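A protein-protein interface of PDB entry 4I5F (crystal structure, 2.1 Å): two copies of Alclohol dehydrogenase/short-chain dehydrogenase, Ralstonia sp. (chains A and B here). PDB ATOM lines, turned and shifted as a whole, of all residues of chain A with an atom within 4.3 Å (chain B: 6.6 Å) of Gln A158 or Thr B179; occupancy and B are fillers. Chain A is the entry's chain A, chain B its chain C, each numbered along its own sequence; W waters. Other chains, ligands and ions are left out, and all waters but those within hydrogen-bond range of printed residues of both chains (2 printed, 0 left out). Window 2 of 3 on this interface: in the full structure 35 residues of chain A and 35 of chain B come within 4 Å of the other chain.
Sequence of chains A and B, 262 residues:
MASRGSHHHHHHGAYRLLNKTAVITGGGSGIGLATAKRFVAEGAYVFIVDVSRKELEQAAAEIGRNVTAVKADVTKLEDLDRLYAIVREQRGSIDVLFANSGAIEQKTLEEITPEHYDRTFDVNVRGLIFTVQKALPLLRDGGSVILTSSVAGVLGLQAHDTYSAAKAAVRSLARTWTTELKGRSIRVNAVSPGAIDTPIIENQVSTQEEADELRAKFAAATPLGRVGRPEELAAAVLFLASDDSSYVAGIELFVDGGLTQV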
ATOM      1  N   THR A 108     -19.571   6.090   2.279  1.00  0.00           N
ATOM      2  CA  THR A 108     -20.473   7.056   2.950  1.00  0.00           C
ATOM      3  C   THR A 108     -21.463   6.303   3.853  1.00  0.00           C
ATOM      4  O   THR A 108     -21.603   5.080   3.707  1.00  0.00           O
ATOM      5  CB  THR A 108     -21.279   7.867   1.938  1.00  0.00           C
ATOM      6  OG1 THR A 108     -22.097   6.955   1.210  1.00  0.00           O
ATOM      7  CG2 THR A 108     -20.355   8.617   1.007  1.00  0.00           C
ATOM      8  N   GLY A 156     -13.987  15.194  10.167  1.00  0.00           N
ATOM      9  CA  GLY A 156     -15.220  14.719   9.519  1.00  0.00           C
ATOM     10  C   GLY A 156     -14.863  14.572   8.022  1.00  0.00           C
ATOM     11  O   GLY A 156     -15.062  15.506   7.207  1.00  0.00           O
ATOM     12  N   LEU A 157     -14.313  13.400   7.661  1.00  0.00           N
ATOM     13  CA  LEU A 157     -13.888  13.180   6.264  1.00  0.00           C
ATOM     14  C   LEU A 157     -14.981  12.407   5.509  1.00  0.00           C
ATOM     15  O   LEU A 157     -15.511  11.416   5.996  1.00  0.00           O
ATOM     16  CB  LEU A 157     -12.521  12.495   6.214  1.00  0.00           C
ATOM     17  CG  LEU A 157     -11.338  13.304   6.881  1.00  0.00           C
ATOM     18  CD1 LEU A 157     -10.099  12.435   7.154  1.00  0.00           C
ATOM     19  CD2 LEU A 157     -10.928  14.585   6.170  1.00  0.00           C
ATOM     20  N   GLN A 158     -15.300  12.876   4.314  1.00  0.00           N
ATOM     21  CA  GLN A 158     -16.243  12.214   3.462  1.00  0.00           C
ATOM     22  C   GLN A 158     -15.913  10.759   3.417  1.00  0.00           C
ATOM     23  O   GLN A 158     -14.758  10.419   3.283  1.00  0.00           O
ATOM     24  CB  GLN A 158     -16.218  12.828   2.038  1.00  0.00           C
ATOM     25  CG  GLN A 158     -17.330  12.311   1.106  1.00  0.00           C
ATOM     26  CD  GLN A 158     -18.743  12.775   1.531  1.00  0.00           C
ATOM     27  OE1 GLN A 158     -18.912  13.701   2.353  1.00  0.00           O
ATOM     28  NE2 GLN A 158     -19.749  12.078   1.048  1.00  0.00           N
ATOM     29  N   ALA A 159     -16.922   9.907   3.570  1.00  0.00           N
ATOM     30  CA  ALA A 159     -16.798   8.440   3.402  1.00  0.00           C
ATOM     31  C   ALA A 159     -15.802   7.750   4.391  1.00  0.00           C
ATOM     32  O   ALA A 159     -15.381   6.625   4.167  1.00  0.00           O
ATOM     33  CB  ALA A 159     -16.446   8.102   1.951  1.00  0.00           C
ATOM     34  N   HIS A 160     -15.410   8.411   5.466  1.00  0.00           N
ATOM     35  CA  HIS A 160     -14.472   7.745   6.423  1.00  0.00           C
ATOM     36  C   HIS A 160     -15.201   7.308   7.656  1.00  0.00           C
ATOM     37  O   HIS A 160     -14.582   7.156   8.744  1.00  0.00           O
ATOM     38  CB  HIS A 160     -13.323   8.711   6.840  1.00  0.00           C
ATOM     39  CG  HIS A 160     -12.289   8.930   5.734  1.00  0.00           C
ATOM     40  ND1 HIS A 160     -12.618   9.437   4.486  1.00  0.00           N
ATOM     41  CD2 HIS A 160     -10.911   8.677   5.701  1.00  0.00           C
ATOM     42  CE1 HIS A 160     -11.499   9.480   3.728  1.00  0.00           C
ATOM     43  NE2 HIS A 160     -10.472   8.998   4.458  1.00  0.00           N
ATOM     44  N   LEU B 173     -18.643  10.087  14.662  1.00  0.00           N
ATOM     45  CA  LEU B 173     -19.665  10.057  13.687  1.00  0.00           C
ATOM     46  C   LEU B 173     -20.444  11.417  13.452  1.00  0.00           C
ATOM     47  O   LEU B 173     -20.747  11.738  12.335  1.00  0.00           O
ATOM     48  CB  LEU B 173     -20.642   8.931  14.048  1.00  0.00           C
ATOM     49  CG  LEU B 173     -20.003   7.567  13.919  1.00  0.00           C
ATOM     50  CD1 LEU B 173     -20.850   6.495  14.634  1.00  0.00           C
ATOM     51  CD2 LEU B 173     -19.693   7.158  12.455  1.00  0.00           C
ATOM     52  N   ALA B 174     -20.706  12.185  14.502  1.00  0.00           N
ATOM     53  CA  ALA B 174     -21.282  13.505  14.395  1.00  0.00           C
ATOM     54  C   ALA B 174     -20.384  14.366  13.501  1.00  0.00           C
ATOM     55  O   ALA B 174     -20.868  15.193  12.683  1.00  0.00           O
ATOM     56  CB  ALA B 174     -21.499  14.152  15.761  1.00  0.00           C
ATOM     57  N   ARG B 175     -19.102  14.096  13.499  1.00  0.00           N
ATOM     58  CA  ARG B 175     -18.268  14.893  12.549  1.00  0.00           C
ATOM     59  C   ARG B 175     -18.399  14.486  11.115  1.00  0.00           C
ATOM     60  O   ARG B 175     -18.527  15.355  10.222  1.00  0.00           O
ATOM     61  CB  ARG B 175     -16.769  14.963  12.907  1.00  0.00           C
ATOM     62  CG  ARG B 175     -16.440  15.041  14.400  1.00  0.00           C
ATOM     63  CD  ARG B 175     -14.918  15.302  14.513  1.00  0.00           C
ATOM     64  NE  ARG B 175     -14.310  15.234  15.874  1.00  0.00           N
ATOM     65  CZ  ARG B 175     -13.803  16.302  16.513  1.00  0.00           C
ATOM     66  NH1 ARG B 175     -13.969  17.524  16.007  1.00  0.00           N
ATOM     67  NH2 ARG B 175     -13.220  16.151  17.710  1.00  0.00           N
ATOM     68  N   THR B 176     -18.304  13.175  10.884  1.00  0.00           N
ATOM     69  CA  THR B 176     -18.306  12.663   9.519  1.00  0.00           C
ATOM     70  C   THR B 176     -19.714  12.965   8.924  1.00  0.00           C
ATOM     71  O   THR B 176     -19.821  13.391   7.786  1.00  0.00           O
ATOM     72  CB  THR B 176     -17.999  11.164   9.516  1.00  0.00           C
ATOM     73  OG1 THR B 176     -16.791  10.914  10.289  1.00  0.00           O
ATOM     74  CG2 THR B 176     -17.896  10.681   8.109  1.00  0.00           C
ATOM     75  N   TRP B 177     -20.759  12.762   9.721  1.00  0.00           N
ATOM     76  CA  TRP B 177     -22.125  13.034   9.260  1.00  0.00           C
ATOM     77  C   TRP B 177     -22.408  14.500   9.032  1.00  0.00           C
ATOM     78  O   TRP B 177     -23.128  14.839   8.118  1.00  0.00           O
ATOM     79  CB  TRP B 177     -23.204  12.374  10.111  1.00  0.00           C
ATOM     80  CG  TRP B 177     -23.019  10.869  10.140  1.00  0.00           C
ATOM     81  CD1 TRP B 177     -22.329  10.081   9.209  1.00  0.00           C
ATOM     82  CD2 TRP B 177     -23.498   9.941  11.155  1.00  0.00           C
ATOM     83  NE1 TRP B 177     -22.357   8.750   9.563  1.00  0.00           N
ATOM     84  CE2 TRP B 177     -23.092   8.576  10.693  1.00  0.00           C
ATOM     85  CE3 TRP B 177     -24.218  10.068  12.342  1.00  0.00           C
ATOM     86  CZ2 TRP B 177     -23.371   7.437  11.427  1.00  0.00           C
ATOM     87  CZ3 TRP B 177     -24.519   8.883  13.054  1.00  0.00           C
ATOM     88  CH2 TRP B 177     -24.090   7.611  12.623  1.00  0.00           C
ATOM     89  N   THR B 178     -21.790  15.354   9.839  1.00  0.00           N
ATOM     90  CA  THR B 178     -21.851  16.758   9.546  1.00  0.00           C
ATOM     91  C   THR B 178     -21.376  17.004   8.099  1.00  0.00           C
ATOM     92  O   THR B 178     -21.943  17.821   7.389  1.00  0.00           O
ATOM     93  CB  THR B 178     -20.999  17.607  10.525  1.00  0.00           C
ATOM     94  OG1 THR B 178     -21.667  17.618  11.787  1.00  0.00           O
ATOM     95  CG2 THR B 178     -20.912  19.024  10.042  1.00  0.00           C
ATOM     96  N   THR B 179     -20.315  16.321   7.699  1.00  0.00           N
ATOM     97  CA  THR B 179     -19.708  16.614   6.362  1.00  0.00           C
ATOM     98  C   THR B 179     -20.584  15.941   5.319  1.00  0.00           C
ATOM     99  O   THR B 179     -20.879  16.561   4.312  1.00  0.00           O
ATOM    100  CB  THR B 179     -18.244  16.126   6.260  1.00  0.00           C
ATOM    101  OG1 THR B 179     -17.387  17.098   6.874  1.00  0.00           O
ATOM    102  CG2 THR B 179     -17.798  15.930   4.790  1.00  0.00           C
ATOM    103  N   GLU B 180     -21.026  14.713   5.581  1.00  0.00           N
ATOM    104  CA  GLU B 180     -21.832  13.983   4.591  1.00  0.00           C
ATOM    105  C   GLU B 180     -23.258  14.511   4.377  1.00  0.00           C
ATOM    106  O   GLU B 180     -23.804  14.330   3.335  1.00  0.00           O
ATOM    107  CB  GLU B 180     -21.886  12.501   4.930  1.00  0.00           C
ATOM    108  CG  GLU B 180     -20.510  11.842   4.691  1.00  0.00           C
ATOM    109  CD  GLU B 180     -20.458  10.336   4.849  1.00  0.00           C
ATOM    110  OE1 GLU B 180     -21.510   9.639   5.026  1.00  0.00           O
ATOM    111  OE2 GLU B 180     -19.325   9.815   4.756  1.00  0.00           O
ATOM    112  N   LEU B 181     -23.887  15.093   5.395  1.00  0.00           N
ATOM    113  CA  LEU B 181     -25.248  15.543   5.230  1.00  0.00           C
ATOM    114  C   LEU B 181     -25.383  17.051   4.956  1.00  0.00           C
ATOM    115  O   LEU B 181     -26.465  17.525   4.771  1.00  0.00           O
ATOM    116  CB  LEU B 181     -26.055  15.101   6.477  1.00  0.00           C
ATOM    117  CG  LEU B 181     -26.086  13.545   6.574  1.00  0.00           C
ATOM    118  CD1 LEU B 181     -26.860  13.194   7.819  1.00  0.00           C
ATOM    119  CD2 LEU B 181     -26.698  12.841   5.354  1.00  0.00           C
ATOM    120  N   LYS B 182     -24.287  17.804   4.944  1.00  0.00           N
ATOM    121  CA  LYS B 182     -24.377  19.251   4.815  1.00  0.00           C
ATOM    122  C   LYS B 182     -25.146  19.621   3.495  1.00  0.00           C
ATOM    123  O   LYS B 182     -25.825  20.648   3.419  1.00  0.00           O
ATOM    124  CB  LYS B 182     -22.962  19.832   4.825  1.00  0.00           C
ATOM    125  CG  LYS B 182     -22.190  19.695   3.486  1.00  0.00           C
ATOM    126  CD  LYS B 182     -20.682  19.802   3.725  1.00  0.00           C
ATOM    127  CE  LYS B 182     -19.807  19.624   2.464  1.00  0.00           C
ATOM    128  NZ  LYS B 182     -18.382  19.830   2.935  1.00  0.00           N
ATOM    129  N   GLY B 183     -25.064  18.739   2.488  1.00  0.00           N
ATOM    130  CA  GLY B 183     -25.659  18.977   1.151  1.00  0.00           C
ATOM    131  C   GLY B 183     -27.172  19.108   1.334  1.00  0.00           C
ATOM    132  O   GLY B 183     -27.848  19.678   0.493  1.00  0.00           O
HETATM  133  O   HOH W   1     -22.585  12.841   1.416  1.00  0.00           O
HETATM  134  O   HOH W   2     -14.062  11.574   9.647  1.00  0.00           O
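No position is printed for both chains. Of the 8 pairs that touch across the chains among the printed residues, none has its exchanged pair printed and touching as well.
Of the printed residues of chain B, Leu A157 touches Thr B176. Of chain B, only Thr B179 (3.5 Å) and Glu B180 (3.4 Å) come within 4 Å of Gln A158. Printed residues of chain A within 4 Å of Arg B175: Gly A156 (3.4 Å). Of the printed residues of chain A, Thr B176 touches Gly A156 and Leu A157. Thr B179 touches just these residues of chain A: Gly A156 and Gln A158. The nearest residue of chain B that does not touch Gln A158 is Thr B176 (5.1 Å).
ND1 of His A160 sits at hydrogen-bond distance from O of Gln A158, 2.6 Å away.
The backbone carbonyl oxygen (O) of Gly A156 lies within hydrogen-bond range of the side-chain hydroxyl (OG1) of Thr B179 (2.8 Å). The backbone NH (N) of Ala A159 sits at hydrogen-bond distance from the side-chain carboxylate (OE2) of Glu B180 (2.7 Å).
Of the 6 printed residues of chain A, 5 touch a printed residue of chain B. Of the 11 printed residues of chain B, 4 touch a printed residue of chain A. Printed residues of chain B that touch a printed residue of chain A: Arg B175, Thr B176, Thr B179 and Glu B180.
Thr A108 touches Glu B180 (CA to OE1, 3.5 Å). O of Arg B175 touches CA of Gly A156 (3.4 Å). CA of Gly A156 touches CA of Thr B176, 3.7 Å away. Thr B176 touches Leu A157. CG2 of Thr B179 touches OE1 of Gln A158 (3.5 Å). Gln A158 touches Glu B180 (OE1 to CG, 3.4 Å).
Water W2 lies within hydrogen-bond range of N of Leu A157 (2.7 Å) and OG1 of Thr B176 (2.9 Å). Water W1 bridges the backbone carbonyl oxygen of Glu B180 (2.7 Å) and the side-chain amide nitrogen of Gln A158 (3.0 Å).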
